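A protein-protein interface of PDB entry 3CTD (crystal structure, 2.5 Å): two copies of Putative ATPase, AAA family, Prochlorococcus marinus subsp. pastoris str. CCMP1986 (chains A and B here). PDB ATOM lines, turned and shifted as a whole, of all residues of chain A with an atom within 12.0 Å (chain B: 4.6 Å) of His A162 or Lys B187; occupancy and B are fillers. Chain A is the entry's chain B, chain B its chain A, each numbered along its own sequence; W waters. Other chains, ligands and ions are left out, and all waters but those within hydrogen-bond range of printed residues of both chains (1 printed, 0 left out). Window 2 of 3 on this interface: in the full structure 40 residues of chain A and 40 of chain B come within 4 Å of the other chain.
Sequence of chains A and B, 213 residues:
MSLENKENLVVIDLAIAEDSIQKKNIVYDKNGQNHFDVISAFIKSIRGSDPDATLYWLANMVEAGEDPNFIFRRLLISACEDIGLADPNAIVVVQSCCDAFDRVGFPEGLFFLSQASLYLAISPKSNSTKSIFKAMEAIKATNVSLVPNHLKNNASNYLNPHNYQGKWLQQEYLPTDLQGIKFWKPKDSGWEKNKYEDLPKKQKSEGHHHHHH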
ATOM      1  N   TYR A 158       6.868  24.765  18.689  1.00  0.00           N
ATOM      2  CA  TYR A 158       7.832  24.033  19.521  1.00  0.00           C
ATOM      3  C   TYR A 158       7.512  22.571  19.451  1.00  0.00           C
ATOM      4  O   TYR A 158       6.337  22.215  19.558  1.00  0.00           O
ATOM      5  CB  TYR A 158       7.744  24.484  20.990  1.00  0.00           C
ATOM      6  CG  TYR A 158       8.507  23.602  21.948  1.00  0.00           C
ATOM      7  CD1 TYR A 158       9.914  23.485  21.850  1.00  0.00           C
ATOM      8  CD2 TYR A 158       7.844  22.864  22.961  1.00  0.00           C
ATOM      9  CE1 TYR A 158      10.658  22.670  22.721  1.00  0.00           C
ATOM     10  CE2 TYR A 158       8.608  22.049  23.870  1.00  0.00           C
ATOM     11  CZ  TYR A 158      10.006  21.970  23.728  1.00  0.00           C
ATOM     12  OH  TYR A 158      10.783  21.184  24.569  1.00  0.00           O
ATOM     13  N   LEU A 159       8.515  21.713  19.256  1.00  0.00           N
ATOM     14  CA  LEU A 159       8.271  20.250  19.438  1.00  0.00           C
ATOM     15  C   LEU A 159       8.919  19.667  20.715  1.00  0.00           C
ATOM     16  O   LEU A 159      10.019  20.049  21.117  1.00  0.00           O
ATOM     17  CB  LEU A 159       8.641  19.423  18.199  1.00  0.00           C
ATOM     18  CG  LEU A 159       7.807  19.857  16.974  1.00  0.00           C
ATOM     19  CD1 LEU A 159       8.536  19.539  15.657  1.00  0.00           C
ATOM     20  CD2 LEU A 159       6.365  19.303  16.994  1.00  0.00           C
ATOM     21  N   ASN A 160       8.214  18.750  21.363  1.00  0.00           N
ATOM     22  CA  ASN A 160       8.618  18.312  22.666  1.00  0.00           C
ATOM     23  C   ASN A 160       9.271  16.957  22.540  1.00  0.00           C
ATOM     24  O   ASN A 160       8.631  15.988  22.098  1.00  0.00           O
ATOM     25  CB  ASN A 160       7.391  18.242  23.580  1.00  0.00           C
ATOM     26  CG  ASN A 160       7.739  18.117  25.051  1.00  0.00           C
ATOM     27  OD1 ASN A 160       8.535  17.248  25.471  1.00  0.00           O
ATOM     28  ND2 ASN A 160       7.116  18.976  25.854  1.00  0.00           N
ATOM     29  N   PRO A 161      10.551  16.889  22.931  1.00  0.00           N
ATOM     30  CA  PRO A 161      11.301  15.632  22.917  1.00  0.00           C
ATOM     31  C   PRO A 161      10.576  14.461  23.620  1.00  0.00           C
ATOM     32  O   PRO A 161      10.820  13.328  23.234  1.00  0.00           O
ATOM     33  CB  PRO A 161      12.616  15.987  23.627  1.00  0.00           C
ATOM     34  CG  PRO A 161      12.729  17.499  23.479  1.00  0.00           C
ATOM     35  CD  PRO A 161      11.353  18.047  23.385  1.00  0.00           C
ATOM     36  N   HIS A 162       9.716  14.727  24.614  1.00  0.00           N
ATOM     37  CA  HIS A 162       8.967  13.672  25.295  1.00  0.00           C
ATOM     38  C   HIS A 162       7.862  13.079  24.422  1.00  0.00           C
ATOM     39  O   HIS A 162       7.379  11.977  24.689  1.00  0.00           O
ATOM     40  CB  HIS A 162       8.264  14.190  26.554  1.00  0.00           C
ATOM     41  CG  HIS A 162       9.184  14.680  27.623  1.00  0.00           C
ATOM     42  ND1 HIS A 162      10.245  13.932  28.096  1.00  0.00           N
ATOM     43  CD2 HIS A 162       9.196  15.842  28.321  1.00  0.00           C
ATOM     44  CE1 HIS A 162      10.891  14.625  29.016  1.00  0.00           C
ATOM     45  NE2 HIS A 162      10.268  15.782  29.178  1.00  0.00           N
ATOM     46  N   ASN A 163       7.397  13.826  23.420  1.00  0.00           N
ATOM     47  CA  ASN A 163       6.365  13.298  22.518  1.00  0.00           C
ATOM     48  C   ASN A 163       7.035  12.565  21.331  1.00  0.00           C
ATOM     49  O   ASN A 163       6.380  12.036  20.446  1.00  0.00           O
ATOM     50  CB  ASN A 163       5.430  14.418  22.026  1.00  0.00           C
ATOM     51  CG  ASN A 163       4.592  15.061  23.162  1.00  0.00           C
ATOM     52  OD1 ASN A 163       4.068  14.370  24.048  1.00  0.00           O
ATOM     53  ND2 ASN A 163       4.462  16.400  23.122  1.00  0.00           N
ATOM     54  N   TYR A 164       8.357  12.534  21.310  1.00  0.00           N
ATOM     55  CA  TYR A 164       9.028  12.226  20.062  1.00  0.00           C
ATOM     56  C   TYR A 164       9.175  10.732  19.859  1.00  0.00           C
ATOM     57  O   TYR A 164       9.779  10.030  20.678  1.00  0.00           O
ATOM     58  CB  TYR A 164      10.374  12.933  19.996  1.00  0.00           C
ATOM     59  CG  TYR A 164      11.079  12.839  18.676  1.00  0.00           C
ATOM     60  CD1 TYR A 164      10.581  13.496  17.555  1.00  0.00           C
ATOM     61  CD2 TYR A 164      12.266  12.089  18.539  1.00  0.00           C
ATOM     62  CE1 TYR A 164      11.243  13.416  16.329  1.00  0.00           C
ATOM     63  CE2 TYR A 164      12.910  12.012  17.334  1.00  0.00           C
ATOM     64  CZ  TYR A 164      12.392  12.677  16.228  1.00  0.00           C
ATOM     65  OH  TYR A 164      13.057  12.621  15.016  1.00  0.00           O
ATOM     66  N   GLN A 165       8.607  10.249  18.755  1.00  0.00           N
ATOM     67  CA  GLN A 165       8.640   8.828  18.441  1.00  0.00           C
ATOM     68  C   GLN A 165       9.937   8.366  17.786  1.00  0.00           C
ATOM     69  O   GLN A 165      10.104   7.178  17.528  1.00  0.00           O
ATOM     70  CB  GLN A 165       7.438   8.430  17.594  1.00  0.00           C
ATOM     71  CG  GLN A 165       6.166   8.331  18.386  1.00  0.00           C
ATOM     72  CD  GLN A 165       6.352   7.504  19.674  1.00  0.00           C
ATOM     73  OE1 GLN A 165       6.868   6.365  19.639  1.00  0.00           O
ATOM     74  NE2 GLN A 165       5.944   8.078  20.817  1.00  0.00           N
ATOM     75  N   GLY A 166      10.850   9.293  17.515  1.00  0.00           N
ATOM     76  CA  GLY A 166      12.139   8.935  16.904  1.00  0.00           C
ATOM     77  C   GLY A 166      13.263   8.738  17.915  1.00  0.00           C
ATOM     78  O   GLY A 166      13.018   8.536  19.108  1.00  0.00           O
ATOM     79  N   LYS A 167      14.497   8.770  17.425  1.00  0.00           N
ATOM     80  CA  LYS A 167      15.660   8.498  18.251  1.00  0.00           C
ATOM     81  C   LYS A 167      16.257   9.821  18.736  1.00  0.00           C
ATOM     82  O   LYS A 167      16.589   9.967  19.896  1.00  0.00           O
ATOM     83  CB  LYS A 167      16.700   7.639  17.496  1.00  0.00           C
ATOM     84  N   TRP A 168      16.387  10.810  17.876  1.00  0.00           N
ATOM     85  CA  TRP A 168      16.820  12.101  18.401  1.00  0.00           C
ATOM     86  C   TRP A 168      16.050  13.251  17.742  1.00  0.00           C
ATOM     87  O   TRP A 168      16.079  13.380  16.528  1.00  0.00           O
ATOM     88  CB  TRP A 168      18.338  12.283  18.231  1.00  0.00           C
ATOM     89  CG  TRP A 168      18.750  13.721  18.464  1.00  0.00           C
ATOM     90  CD1 TRP A 168      18.416  14.506  19.553  1.00  0.00           C
ATOM     91  CD2 TRP A 168      19.543  14.565  17.590  1.00  0.00           C
ATOM     92  NE1 TRP A 168      18.965  15.767  19.412  1.00  0.00           N
ATOM     93  CE2 TRP A 168      19.660  15.831  18.223  1.00  0.00           C
ATOM     94  CE3 TRP A 168      20.163  14.370  16.352  1.00  0.00           C
ATOM     95  CZ2 TRP A 168      20.377  16.899  17.644  1.00  0.00           C
ATOM     96  CZ3 TRP A 168      20.874  15.424  15.783  1.00  0.00           C
ATOM     97  CH2 TRP A 168      20.974  16.674  16.430  1.00  0.00           C
ATOM     98  N   LEU A 169      15.362  14.076  18.530  1.00  0.00           N
ATOM     99  CA  LEU A 169      14.629  15.218  17.947  1.00  0.00           C
ATOM    100  C   LEU A 169      15.656  16.257  17.515  1.00  0.00           C
ATOM    101  O   LEU A 169      16.322  16.866  18.350  1.00  0.00           O
ATOM    102  CB  LEU A 169      13.619  15.804  18.935  1.00  0.00           C
ATOM    103  CG  LEU A 169      12.832  17.066  18.531  1.00  0.00           C
ATOM    104  CD1 LEU A 169      12.131  16.824  17.231  1.00  0.00           C
ATOM    105  CD2 LEU A 169      11.815  17.510  19.616  1.00  0.00           C
ATOM    106  N   GLN A 170      15.818  16.445  16.209  1.00  0.00           N
ATOM    107  CA  GLN A 170      16.704  17.517  15.756  1.00  0.00           C
ATOM    108  C   GLN A 170      15.988  18.906  15.809  1.00  0.00           C
ATOM    109  O   GLN A 170      15.108  19.204  14.993  1.00  0.00           O
ATOM    110  CB  GLN A 170      17.295  17.159  14.382  1.00  0.00           C
ATOM    111  CG  GLN A 170      18.084  18.271  13.720  1.00  0.00           C
ATOM    112  CD  GLN A 170      18.786  17.800  12.454  1.00  0.00           C
ATOM    113  OE1 GLN A 170      18.367  16.818  11.836  1.00  0.00           O
ATOM    114  NE2 GLN A 170      19.857  18.492  12.071  1.00  0.00           N
ATOM    115  N   GLN A 171      16.315  19.726  16.814  1.00  0.00           N
ATOM    116  CA  GLN A 171      15.674  21.025  16.961  1.00  0.00           C
ATOM    117  C   GLN A 171      16.713  22.034  17.427  1.00  0.00           C
ATOM    118  O   GLN A 171      17.575  21.711  18.220  1.00  0.00           O
ATOM    119  CB  GLN A 171      14.472  20.932  17.949  1.00  0.00           C
ATOM    120  CG  GLN A 171      13.674  22.227  18.198  1.00  0.00           C
ATOM    121  CD  GLN A 171      12.381  21.966  18.956  1.00  0.00           C
ATOM    122  OE1 GLN A 171      11.317  22.349  18.506  1.00  0.00           O
ATOM    123  NE2 GLN A 171      12.465  21.307  20.119  1.00  0.00           N
ATOM    124  N   TYR A 173      18.392  24.861  19.513  1.00  0.00           N
ATOM    125  CA  TYR A 173      18.312  25.360  20.882  1.00  0.00           C
ATOM    126  C   TYR A 173      19.130  26.617  21.074  1.00  0.00           C
ATOM    127  O   TYR A 173      18.903  27.424  21.998  1.00  0.00           O
ATOM    128  CB  TYR A 173      18.684  24.254  21.890  1.00  0.00           C
ATOM    129  CG  TYR A 173      17.641  23.124  21.880  1.00  0.00           C
ATOM    130  CD1 TYR A 173      16.303  23.391  22.177  1.00  0.00           C
ATOM    131  CD2 TYR A 173      17.984  21.816  21.565  1.00  0.00           C
ATOM    132  CE1 TYR A 173      15.333  22.387  22.148  1.00  0.00           C
ATOM    133  CE2 TYR A 173      17.040  20.804  21.541  1.00  0.00           C
ATOM    134  CZ  TYR A 173      15.705  21.103  21.819  1.00  0.00           C
ATOM    135  OH  TYR A 173      14.715  20.131  21.759  1.00  0.00           O
ATOM    136  N   ARG B  47      15.653  20.214  28.381  1.00  0.00           N
ATOM    137  CA  ARG B  47      14.796  19.089  27.940  1.00  0.00           C
ATOM    138  C   ARG B  47      15.325  18.419  26.683  1.00  0.00           C
ATOM    139  O   ARG B  47      15.177  17.214  26.525  1.00  0.00           O
ATOM    140  CB  ARG B  47      13.332  19.528  27.741  1.00  0.00           C
ATOM    141  CG  ARG B  47      12.431  18.432  27.357  1.00  0.00           C
ATOM    142  CD  ARG B  47      10.974  18.943  27.202  1.00  0.00           C
ATOM    143  NE  ARG B  47      10.551  19.614  28.423  1.00  0.00           N
ATOM    144  CZ  ARG B  47      10.020  20.832  28.461  1.00  0.00           C
ATOM    145  NH1 ARG B  47       9.786  21.506  27.344  1.00  0.00           N
ATOM    146  NH2 ARG B  47       9.695  21.372  29.618  1.00  0.00           N
ATOM    147  N   GLU B  81      10.027  16.871  36.357  1.00  0.00           N
ATOM    148  CA  GLU B  81       9.119  16.726  35.230  1.00  0.00           C
ATOM    149  C   GLU B  81       9.843  16.239  33.939  1.00  0.00           C
ATOM    150  O   GLU B  81       9.244  15.555  33.090  1.00  0.00           O
ATOM    151  CB  GLU B  81       8.297  17.988  35.049  1.00  0.00           C
ATOM    152  CG  GLU B  81       7.619  18.122  33.700  1.00  0.00           C
ATOM    153  CD  GLU B  81       7.098  19.554  33.381  1.00  0.00           C
ATOM    154  OE1 GLU B  81       6.354  19.670  32.381  1.00  0.00           O
ATOM    155  OE2 GLU B  81       7.424  20.547  34.094  1.00  0.00           O
ATOM    156  N   ASP B  82      11.149  16.507  33.833  1.00  0.00           N
ATOM    157  CA  ASP B  82      11.874  16.239  32.573  1.00  0.00           C
ATOM    158  C   ASP B  82      12.902  15.116  32.671  1.00  0.00           C
ATOM    159  O   ASP B  82      13.174  14.443  31.684  1.00  0.00           O
ATOM    160  CB  ASP B  82      12.483  17.531  32.025  1.00  0.00           C
ATOM    161  CG  ASP B  82      11.391  18.532  31.522  1.00  0.00           C
ATOM    162  OD1 ASP B  82      10.491  18.154  30.723  1.00  0.00           O
ATOM    163  OD2 ASP B  82      11.450  19.717  31.892  1.00  0.00           O
ATOM    164  N   LYS B 125      16.296  11.425  30.079  1.00  0.00           N
ATOM    165  CA  LYS B 125      15.055  12.188  30.192  1.00  0.00           C
ATOM    166  C   LYS B 125      13.868  11.275  30.304  1.00  0.00           C
ATOM    167  O   LYS B 125      13.850  10.232  29.651  1.00  0.00           O
ATOM    168  CB  LYS B 125      14.866  13.050  28.916  1.00  0.00           C
ATOM    169  CG  LYS B 125      15.959  14.197  28.788  1.00  0.00           C
ATOM    170  CD  LYS B 125      16.312  14.901  30.152  1.00  0.00           C
ATOM    171  CE  LYS B 125      17.027  16.210  29.916  1.00  0.00           C
ATOM    172  NZ  LYS B 125      18.418  16.013  29.329  1.00  0.00           N
ATOM    173  N   SER B 126      12.857  11.698  31.077  1.00  0.00           N
ATOM    174  CA  SER B 126      11.563  11.050  31.092  1.00  0.00           C
ATOM    175  C   SER B 126      10.493  11.969  31.680  1.00  0.00           C
ATOM    176  O   SER B 126      10.730  12.647  32.681  1.00  0.00           O
ATOM    177  CB  SER B 126      11.634   9.802  31.978  1.00  0.00           C
ATOM    178  OG  SER B 126      10.319   9.358  32.337  1.00  0.00           O
ATOM    179  N   ASN B 127       9.289  11.943  31.108  1.00  0.00           N
ATOM    180  CA  ASN B 127       8.188  12.662  31.713  1.00  0.00           C
ATOM    181  C   ASN B 127       7.187  11.707  32.371  1.00  0.00           C
ATOM    182  O   ASN B 127       6.063  12.087  32.646  1.00  0.00           O
ATOM    183  CB  ASN B 127       7.475  13.521  30.684  1.00  0.00           C
ATOM    184  CG  ASN B 127       6.747  12.676  29.681  1.00  0.00           C
ATOM    185  OD1 ASN B 127       7.091  11.506  29.482  1.00  0.00           O
ATOM    186  ND2 ASN B 127       5.730  13.233  29.062  1.00  0.00           N
ATOM    187  N   LYS B 185       3.468   5.502  32.197  1.00  0.00           N
ATOM    188  CA  LYS B 185       4.198   5.305  30.941  1.00  0.00           C
ATOM    189  C   LYS B 185       5.715   5.564  31.095  1.00  0.00           C
ATOM    190  O   LYS B 185       6.159   6.716  30.961  1.00  0.00           O
ATOM    191  CB  LYS B 185       3.620   6.258  29.872  1.00  0.00           C
ATOM    192  N   PRO B 186       6.505   4.500  31.371  1.00  0.00           N
ATOM    193  CA  PRO B 186       7.980   4.581  31.466  1.00  0.00           C
ATOM    194  C   PRO B 186       8.653   4.795  30.091  1.00  0.00           C
ATOM    195  O   PRO B 186       8.166   4.266  29.114  1.00  0.00           O
ATOM    196  CB  PRO B 186       8.368   3.230  32.094  1.00  0.00           C
ATOM    197  CG  PRO B 186       7.249   2.336  31.776  1.00  0.00           C
ATOM    198  CD  PRO B 186       5.995   3.141  31.625  1.00  0.00           C
ATOM    199  N   LYS B 187       9.798   5.495  30.026  1.00  0.00           N
ATOM    200  CA  LYS B 187      10.352   5.985  28.745  1.00  0.00           C
ATOM    201  C   LYS B 187      11.643   5.326  28.274  1.00  0.00           C
ATOM    202  O   LYS B 187      12.060   4.317  28.827  1.00  0.00           O
ATOM    203  CB  LYS B 187      10.548   7.508  28.776  1.00  0.00           C
ATOM    204  CG  LYS B 187       9.236   8.296  28.811  1.00  0.00           C
ATOM    205  CD  LYS B 187       8.189   7.707  27.816  1.00  0.00           C
ATOM    206  CE  LYS B 187       7.376   8.809  27.118  1.00  0.00           C
ATOM    207  NZ  LYS B 187       8.289   9.714  26.331  1.00  0.00           N
ATOM    208  N   GLU B 192      14.370   4.145  35.652  1.00  0.00           N
ATOM    209  CA  GLU B 192      13.030   3.542  35.510  1.00  0.00           C
ATOM    210  C   GLU B 192      12.994   2.400  34.500  1.00  0.00           C
ATOM    211  O   GLU B 192      12.154   1.497  34.606  1.00  0.00           O
ATOM    212  CB  GLU B 192      11.930   4.572  35.174  1.00  0.00           C
ATOM    213  CG  GLU B 192      12.024   5.223  33.808  1.00  0.00           C
ATOM    214  CD  GLU B 192      10.885   6.182  33.488  1.00  0.00           C
ATOM    215  OE1 GLU B 192       9.926   6.364  34.279  1.00  0.00           O
ATOM    216  OE2 GLU B 192      10.948   6.787  32.406  1.00  0.00           O
HETATM  217  O   HOH W   1      10.109  11.234  27.894  1.00  0.00           O
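A ring nitrogen (NE2) of His A162 sits at hydrogen-bond distance from the side-chain carboxylate of Asp B82 (2.8 Å).
The side-chain hydroxyl of Tyr A158 sits at hydrogen-bond distance from the guanidinium group of Arg B47, 3.0 Å away.
NZ of Lys B187 is in hydrogen-bond range of O of His A162.
The backbone NH (N) of Ser B126 is in hydrogen-bond range of the backbone carbonyl oxygen (O) of Asp B82, 2.8 Å away.
N of Lys B187 lies within hydrogen-bond range of OE2 of Glu B192 (2.9 Å).
The side-chain hydroxyl (OG) of Ser B126 is in hydrogen-bond range of the side-chain carboxylate (OE2) of Glu B192 (2.6 Å).
NE of Arg B47 is in salt-bridge range of OD1 of Asp B82, at 2.7 Å.
The side-chain amide oxygen (OD1) of Asn A160 lies within hydrogen-bond range of the backbone NH (N) of His A162, 2.9 Å away.
Among the printed residues, merely in contact across the chains: Asn A160 with Arg B47 (3.4 Å), Pro A161 with Arg B47 (3.9 Å), His A162 with Arg B47 (3.7 Å), His A162 with Ser B126 (3.8 Å) and His A162 with Asn B127 (3.7 Å).
Of the printed residues of chain B, Tyr A158 touches Arg B47.
Printed residues of chain B within 4 Å of Asn A160: Arg B47.
Printed residues of chain B within 4 Å of Pro A161: Arg B47.
Gln A170 touches none of the printed residues of chain B.
Arg B47 touches just these residues of chain A: Tyr A158, Asn A160, Pro A161 and His A162.
No residue of chain A comes within 4 Å of Glu B81.
No residue of chain A comes within 4 Å of Lys B125.
Of chain A, only His A162 comes within 4 Å of Asn B127.
No residue of chain A comes within 4 Å of Pro B186.
The nearest residue of chain B that does not touch His A162 is Glu B81 (4.1 Å).
The nearest printed residue of chain B that does not touch Asn A160 is Asp B82 (5.7 Å).
Hydrophobic or aromatic side chains of chain A within 4 Å of the printed part of chain B: Tyr A158, Pro A161 and His A162.
Among the printed residues, no Asp or Glu carboxylate lies within 4 Å of a Lys or Arg side-chain nitrogen of the other chain.
No position is printed for both chains.
Water W1 lies within hydrogen-bond range of a ring nitrogen (ND1) of His A162 (2.7 Å), the side-chain amino group (NZ) of Lys B187 (2.8 Å) and the backbone NH (N) of Asn B127 (3.4 Å).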
